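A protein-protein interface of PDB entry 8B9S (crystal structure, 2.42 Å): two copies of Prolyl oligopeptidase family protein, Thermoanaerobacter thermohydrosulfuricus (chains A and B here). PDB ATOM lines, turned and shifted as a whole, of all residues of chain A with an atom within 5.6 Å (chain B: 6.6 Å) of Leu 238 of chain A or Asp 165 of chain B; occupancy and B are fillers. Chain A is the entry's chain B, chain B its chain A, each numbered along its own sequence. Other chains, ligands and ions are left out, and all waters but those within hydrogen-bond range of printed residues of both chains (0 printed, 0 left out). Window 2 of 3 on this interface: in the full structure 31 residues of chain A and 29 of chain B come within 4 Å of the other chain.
OD2 of Asp 165 of chain B sits at hydrogen-bond distance from N of Leu 238 of chain A (2.8 Å). O of Gly 168 of chain B lies close to OE2 of Glu 241 of chain A.
O of Asp 165 of chain B is in hydrogen-bond range of OH of Tyr 154 of chain B, at 2.6 Å. OD1 of Asp 165 of chain B is in hydrogen-bond range of N of Gly 167 of chain B, 2.8 Å away. N of Gly 168 of chain B is in hydrogen-bond range of OD1 of Asp 165 of chain B, at 2.8 Å. O of Phe 235 of chain A is in hydrogen-bond range of N of Glu 241 of chain A (3.4 Å). The side-chain hydroxyl of Ser 237 of chain A sits at hydrogen-bond distance from the backbone NH of Trp 240 of chain A (3.1 Å).
Among the printed residues, merely in contact across the chains: Lys 236 of chain A with Gly 167 of chain B (3.3 Å), Ser 237 of chain A with Asp 165 of chain B (3.3 Å), Ser 237 of chain A with Gly 168 of chain B (3.8 Å), Leu 238 of chain A with His 169 of chain B (3.95 Å) and Leu 238 of chain A with Lys 170 of chain B (3.9 Å).
Of the printed residues of chain B, Leu 238 of chain A touches Asp 165, His 169 and Lys 170. Asp 165 of chain B touches two residues of chain A. Of the printed residues of chain B, Ser 237 of chain A touches Asp 165 (3.3 Å) and Gly 168 (3.8 Å). Of the printed residues of chain A, Gly 168 of chain B touches Ser 237 (3.8 Å) and Glu 241 (3.4 Å). Of the printed residues of chain B, Lys 236 of chain A touches Gly 167. Of the printed residues of chain B, Glu 241 of chain A touches Gly 168. Printed residues of chain A within 4 Å of Lys 170 of chain B: Leu 238 (3.9 Å). The nearest printed residue of chain B that does not touch Ser 237 of chain A is Gly 167 of chain B (4.6 Å).
Hydrophobic or aromatic side chains of chain A within 4 Å of the printed part of chain B: Leu 238. Among the printed residues, no Asp or Glu carboxylate lies within 4 Å of a Lys or Arg side-chain nitrogen of the other chain.
No position is printed for both chains.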
ATOM      1  N   PHE A 235      -9.535  26.314  -4.272  1.00  0.00           N
ATOM      2  CA  PHE A 235      -9.697  25.074  -3.516  1.00  0.00           C
ATOM      3  C   PHE A 235     -10.708  25.281  -2.383  1.00  0.00           C
ATOM      4  O   PHE A 235     -10.457  24.950  -1.216  1.00  0.00           O
ATOM      5  CB  PHE A 235      -8.351  24.583  -2.961  1.00  0.00           C
ATOM      6  CG  PHE A 235      -7.201  24.705  -3.927  1.00  0.00           C
ATOM      7  CD1 PHE A 235      -7.195  24.022  -5.133  1.00  0.00           C
ATOM      8  CD2 PHE A 235      -6.087  25.443  -3.577  1.00  0.00           C
ATOM      9  CE1 PHE A 235      -6.113  24.133  -6.006  1.00  0.00           C
ATOM     10  CE2 PHE A 235      -4.997  25.553  -4.423  1.00  0.00           C
ATOM     11  CZ  PHE A 235      -5.005  24.893  -5.643  1.00  0.00           C
ATOM     12  N   LYS A 236     -11.860  25.852  -2.743  1.00  0.00           N
ATOM     13  CA  LYS A 236     -12.842  26.368  -1.785  1.00  0.00           C
ATOM     14  C   LYS A 236     -13.768  25.242  -1.309  1.00  0.00           C
ATOM     15  O   LYS A 236     -14.949  25.167  -1.644  1.00  0.00           O
ATOM     16  CB  LYS A 236     -13.619  27.521  -2.414  1.00  0.00           C
ATOM     17  CG  LYS A 236     -14.579  28.249  -1.481  1.00  0.00           C
ATOM     18  CD  LYS A 236     -15.398  29.338  -2.210  1.00  0.00           C
ATOM     19  CE  LYS A 236     -14.594  30.614  -2.482  1.00  0.00           C
ATOM     20  NZ  LYS A 236     -15.429  31.746  -3.051  1.00  0.00           N
ATOM     21  N   SER A 237     -13.180  24.312  -0.559  1.00  0.00           N
ATOM     22  CA  SER A 237     -13.924  23.365   0.267  1.00  0.00           C
ATOM     23  C   SER A 237     -12.972  22.858   1.336  1.00  0.00           C
ATOM     24  O   SER A 237     -11.754  23.024   1.234  1.00  0.00           O
ATOM     25  CB  SER A 237     -14.491  22.179  -0.526  1.00  0.00           C
ATOM     26  OG  SER A 237     -13.474  21.247  -0.838  1.00  0.00           O
ATOM     27  N   LEU A 238     -13.543  22.243   2.367  1.00  0.00           N
ATOM     28  CA  LEU A 238     -12.719  21.711   3.448  1.00  0.00           C
ATOM     29  C   LEU A 238     -11.746  20.653   2.918  1.00  0.00           C
ATOM     30  O   LEU A 238     -10.543  20.692   3.205  1.00  0.00           O
ATOM     31  CB  LEU A 238     -13.627  21.154   4.545  1.00  0.00           C
ATOM     32  CG  LEU A 238     -14.487  22.246   5.204  1.00  0.00           C
ATOM     33  CD1 LEU A 238     -15.619  21.652   6.006  1.00  0.00           C
ATOM     34  CD2 LEU A 238     -13.633  23.129   6.109  1.00  0.00           C
ATOM     35  N   GLU A 239     -12.241  19.743   2.078  1.00  0.00           N
ATOM     36  CA  GLU A 239     -11.388  18.677   1.566  1.00  0.00           C
ATOM     37  C   GLU A 239     -10.302  19.229   0.649  1.00  0.00           C
ATOM     38  O   GLU A 239      -9.122  18.875   0.780  1.00  0.00           O
ATOM     39  CB  GLU A 239     -12.241  17.652   0.811  1.00  0.00           C
ATOM     40  CG  GLU A 239     -13.161  16.764   1.645  1.00  0.00           C
ATOM     41  CD  GLU A 239     -14.484  17.416   2.036  1.00  0.00           C
ATOM     42  OE1 GLU A 239     -14.714  18.606   1.712  1.00  0.00           O
ATOM     43  OE2 GLU A 239     -15.315  16.714   2.659  1.00  0.00           O
ATOM     44  N   TRP A 240     -10.682  20.123  -0.270  1.00  0.00           N
ATOM     45  CA  TRP A 240      -9.732  20.654  -1.239  1.00  0.00           C
ATOM     46  C   TRP A 240      -8.642  21.472  -0.559  1.00  0.00           C
ATOM     47  O   TRP A 240      -7.456  21.327  -0.884  1.00  0.00           O
ATOM     48  CB  TRP A 240     -10.468  21.488  -2.280  1.00  0.00           C
ATOM     49  CG  TRP A 240     -11.438  20.699  -3.110  1.00  0.00           C
ATOM     50  CD1 TRP A 240     -11.473  19.336  -3.280  1.00  0.00           C
ATOM     51  CD2 TRP A 240     -12.580  21.220  -3.813  1.00  0.00           C
ATOM     52  NE1 TRP A 240     -12.536  18.989  -4.081  1.00  0.00           N
ATOM     53  CE2 TRP A 240     -13.239  20.122  -4.412  1.00  0.00           C
ATOM     54  CE3 TRP A 240     -13.103  22.507  -4.000  1.00  0.00           C
ATOM     55  CZ2 TRP A 240     -14.391  20.277  -5.197  1.00  0.00           C
ATOM     56  CZ3 TRP A 240     -14.247  22.660  -4.787  1.00  0.00           C
ATOM     57  CH2 TRP A 240     -14.879  21.550  -5.368  1.00  0.00           C
ATOM     58  N   GLU A 241      -9.013  22.338   0.391  1.00  0.00           N
ATOM     59  CA  GLU A 241      -7.979  23.144   1.025  1.00  0.00           C
ATOM     60  C   GLU A 241      -7.110  22.291   1.933  1.00  0.00           C
ATOM     61  O   GLU A 241      -5.907  22.547   2.035  1.00  0.00           O
ATOM     62  CB  GLU A 241      -8.552  24.340   1.797  1.00  0.00           C
ATOM     63  CG  GLU A 241      -9.249  24.046   3.091  1.00  0.00           C
ATOM     64  CD  GLU A 241      -9.525  25.323   3.901  1.00  0.00           C
ATOM     65  OE1 GLU A 241      -9.194  26.435   3.422  1.00  0.00           O
ATOM     66  OE2 GLU A 241     -10.055  25.208   5.032  1.00  0.00           O
ATOM     67  N   LYS A 242      -7.682  21.271   2.587  1.00  0.00           N
ATOM     68  CA  LYS A 242      -6.838  20.357   3.340  1.00  0.00           C
ATOM     69  C   LYS A 242      -5.810  19.699   2.429  1.00  0.00           C
ATOM     70  O   LYS A 242      -4.624  19.627   2.771  1.00  0.00           O
ATOM     71  CB  LYS A 242      -7.680  19.285   4.033  1.00  0.00           C
ATOM     72  CG  LYS A 242      -6.840  18.301   4.864  1.00  0.00           C
ATOM     73  CD  LYS A 242      -7.651  17.089   5.349  1.00  0.00           C
ATOM     74  CE  LYS A 242      -8.499  17.341   6.587  1.00  0.00           C
ATOM     75  NZ  LYS A 242      -7.680  17.343   7.844  1.00  0.00           N
ATOM     76  N   LYS A 243      -6.231  19.235   1.248  1.00  0.00           N
ATOM     77  CA  LYS A 243      -5.268  18.586   0.365  1.00  0.00           C
ATOM     78  C   LYS A 243      -4.189  19.559  -0.080  1.00  0.00           C
ATOM     79  O   LYS A 243      -2.995  19.225  -0.079  1.00  0.00           O
ATOM     80  CB  LYS A 243      -5.942  17.964  -0.852  1.00  0.00           C
ATOM     81  CG  LYS A 243      -4.916  17.156  -1.636  1.00  0.00           C
ATOM     82  CD  LYS A 243      -5.445  16.398  -2.825  1.00  0.00           C
ATOM     83  CE  LYS A 243      -4.282  15.623  -3.460  1.00  0.00           C
ATOM     84  NZ  LYS A 243      -4.691  14.860  -4.666  1.00  0.00           N
ATOM     85  N   TYR B 154     -28.399  21.635   3.648  1.00  0.00           N
ATOM     86  CA  TYR B 154     -27.526  21.927   4.785  1.00  0.00           C
ATOM     87  C   TYR B 154     -28.097  21.374   6.090  1.00  0.00           C
ATOM     88  O   TYR B 154     -27.337  20.906   6.940  1.00  0.00           O
ATOM     89  CB  TYR B 154     -27.292  23.439   4.909  1.00  0.00           C
ATOM     90  CG  TYR B 154     -26.059  23.930   4.197  1.00  0.00           C
ATOM     91  CD1 TYR B 154     -24.981  23.083   3.981  1.00  0.00           C
ATOM     92  CD2 TYR B 154     -25.975  25.230   3.724  1.00  0.00           C
ATOM     93  CE1 TYR B 154     -23.846  23.519   3.327  1.00  0.00           C
ATOM     94  CE2 TYR B 154     -24.836  25.678   3.068  1.00  0.00           C
ATOM     95  CZ  TYR B 154     -23.781  24.822   2.871  1.00  0.00           C
ATOM     96  OH  TYR B 154     -22.653  25.272   2.219  1.00  0.00           O
ATOM     97  N   ILE B 157     -27.259  17.635   6.024  1.00  0.00           N
ATOM     98  CA  ILE B 157     -25.822  17.464   6.210  1.00  0.00           C
ATOM     99  C   ILE B 157     -25.444  17.723   7.665  1.00  0.00           C
ATOM    100  O   ILE B 157     -24.650  16.983   8.256  1.00  0.00           O
ATOM    101  CB  ILE B 157     -25.042  18.373   5.238  1.00  0.00           C
ATOM    102  CG1 ILE B 157     -25.320  17.971   3.789  1.00  0.00           C
ATOM    103  CG2 ILE B 157     -23.550  18.303   5.512  1.00  0.00           C
ATOM    104  CD1 ILE B 157     -24.808  18.962   2.761  1.00  0.00           C
ATOM    105  N   PHE B 163     -21.656  19.325  11.347  1.00  0.00           N
ATOM    106  CA  PHE B 163     -20.998  20.522  10.823  1.00  0.00           C
ATOM    107  C   PHE B 163     -21.314  20.584   9.363  1.00  0.00           C
ATOM    108  O   PHE B 163     -21.615  19.567   8.746  1.00  0.00           O
ATOM    109  CB  PHE B 163     -19.510  20.401  11.137  1.00  0.00           C
ATOM    110  CG  PHE B 163     -18.682  19.510  10.230  1.00  0.00           C
ATOM    111  CD1 PHE B 163     -18.486  19.769   8.887  1.00  0.00           C
ATOM    112  CD2 PHE B 163     -18.260  18.276  10.729  1.00  0.00           C
ATOM    113  CE1 PHE B 163     -17.743  18.915   8.098  1.00  0.00           C
ATOM    114  CE2 PHE B 163     -17.544  17.400   9.929  1.00  0.00           C
ATOM    115  CZ  PHE B 163     -17.287  17.719   8.613  1.00  0.00           C
ATOM    116  N   VAL B 164     -21.200  21.780   8.756  1.00  0.00           N
ATOM    117  CA  VAL B 164     -21.365  21.872   7.310  1.00  0.00           C
ATOM    118  C   VAL B 164     -20.244  22.716   6.729  1.00  0.00           C
ATOM    119  O   VAL B 164     -19.650  23.555   7.398  1.00  0.00           O
ATOM    120  CB  VAL B 164     -22.728  22.447   6.846  1.00  0.00           C
ATOM    121  CG1 VAL B 164     -23.865  21.522   7.221  1.00  0.00           C
ATOM    122  CG2 VAL B 164     -22.949  23.836   7.431  1.00  0.00           C
ATOM    123  N   ASP B 165     -19.954  22.461   5.459  1.00  0.00           N
ATOM    124  CA  ASP B 165     -18.978  23.232   4.704  1.00  0.00           C
ATOM    125  C   ASP B 165     -19.690  24.367   3.981  1.00  0.00           C
ATOM    126  O   ASP B 165     -20.553  24.127   3.125  1.00  0.00           O
ATOM    127  CB  ASP B 165     -18.232  22.318   3.729  1.00  0.00           C
ATOM    128  CG  ASP B 165     -17.074  23.009   3.021  1.00  0.00           C
ATOM    129  OD1 ASP B 165     -16.909  24.240   3.126  1.00  0.00           O
ATOM    130  OD2 ASP B 165     -16.304  22.297   2.350  1.00  0.00           O
ATOM    131  N   ILE B 166     -19.343  25.600   4.345  1.00  0.00           N
ATOM    132  CA  ILE B 166     -19.945  26.761   3.696  1.00  0.00           C
ATOM    133  C   ILE B 166     -18.956  27.432   2.748  1.00  0.00           C
ATOM    134  O   ILE B 166     -19.098  28.619   2.448  1.00  0.00           O
ATOM    135  CB  ILE B 166     -20.515  27.750   4.747  1.00  0.00           C
ATOM    136  CG1 ILE B 166     -19.466  28.207   5.756  1.00  0.00           C
ATOM    137  CG2 ILE B 166     -21.712  27.135   5.474  1.00  0.00           C
ATOM    138  CD1 ILE B 166     -20.017  29.223   6.750  1.00  0.00           C
ATOM    139  N   GLY B 167     -18.003  26.680   2.195  1.00  0.00           N
ATOM    140  CA  GLY B 167     -17.053  27.254   1.257  1.00  0.00           C
ATOM    141  C   GLY B 167     -15.651  27.372   1.807  1.00  0.00           C
ATOM    142  O   GLY B 167     -15.069  28.465   1.821  1.00  0.00           O
ATOM    143  N   GLY B 168     -15.129  26.266   2.337  1.00  0.00           N
ATOM    144  CA  GLY B 168     -13.841  26.301   3.009  1.00  0.00           C
ATOM    145  C   GLY B 168     -13.920  26.765   4.447  1.00  0.00           C
ATOM    146  O   GLY B 168     -12.893  27.146   5.027  1.00  0.00           O
ATOM    147  N   HIS B 169     -15.115  26.767   5.030  1.00  0.00           N
ATOM    148  CA  HIS B 169     -15.312  27.084   6.437  1.00  0.00           C
ATOM    149  C   HIS B 169     -16.194  25.996   7.023  1.00  0.00           C
ATOM    150  O   HIS B 169     -17.163  25.557   6.385  1.00  0.00           O
ATOM    151  CB  HIS B 169     -15.981  28.450   6.647  1.00  0.00           C
ATOM    152  CG  HIS B 169     -15.225  29.595   6.061  1.00  0.00           C
ATOM    153  ND1 HIS B 169     -14.089  30.113   6.641  1.00  0.00           N
ATOM    154  CD2 HIS B 169     -15.451  30.333   4.947  1.00  0.00           C
ATOM    155  CE1 HIS B 169     -13.638  31.112   5.905  1.00  0.00           C
ATOM    156  NE2 HIS B 169     -14.446  31.265   4.872  1.00  0.00           N
ATOM    157  N   LYS B 170     -15.849  25.557   8.231  1.00  0.00           N
ATOM    158  CA  LYS B 170     -16.587  24.509   8.928  1.00  0.00           C
ATOM    159  C   LYS B 170     -17.551  25.162   9.918  1.00  0.00           C
ATOM    160  O   LYS B 170     -17.144  25.621  10.990  1.00  0.00           O
ATOM    161  CB  LYS B 170     -15.591  23.570   9.600  1.00  0.00           C
ATOM    162  CG  LYS B 170     -16.160  22.332  10.233  1.00  0.00           C
ATOM    163  CD  LYS B 170     -15.024  21.521  10.825  1.00  0.00           C
ATOM    164  CE  LYS B 170     -15.558  20.332  11.593  1.00  0.00           C
ATOM    165  NZ  LYS B 170     -14.558  19.471  12.287  1.00  0.00           N
ATOM    166  N   LEU B 171     -18.837  25.177   9.569  1.00  0.00           N
ATOM    167  CA  LEU B 171     -19.881  25.743  10.421  1.00  0.00           C
ATOM    168  C   LEU B 171     -20.393  24.658  11.359  1.00  0.00           C
ATOM    169  O   LEU B 171     -21.053  23.713  10.922  1.00  0.00           O
ATOM    170  CB  LEU B 171     -21.032  26.305   9.592  1.00  0.00           C
ATOM    171  CG  LEU B 171     -22.102  26.904  10.510  1.00  0.00           C
ATOM    172  CD1 LEU B 171     -21.521  28.068  11.268  1.00  0.00           C
ATOM    173  CD2 LEU B 171     -23.339  27.321   9.733  1.00  0.00           C
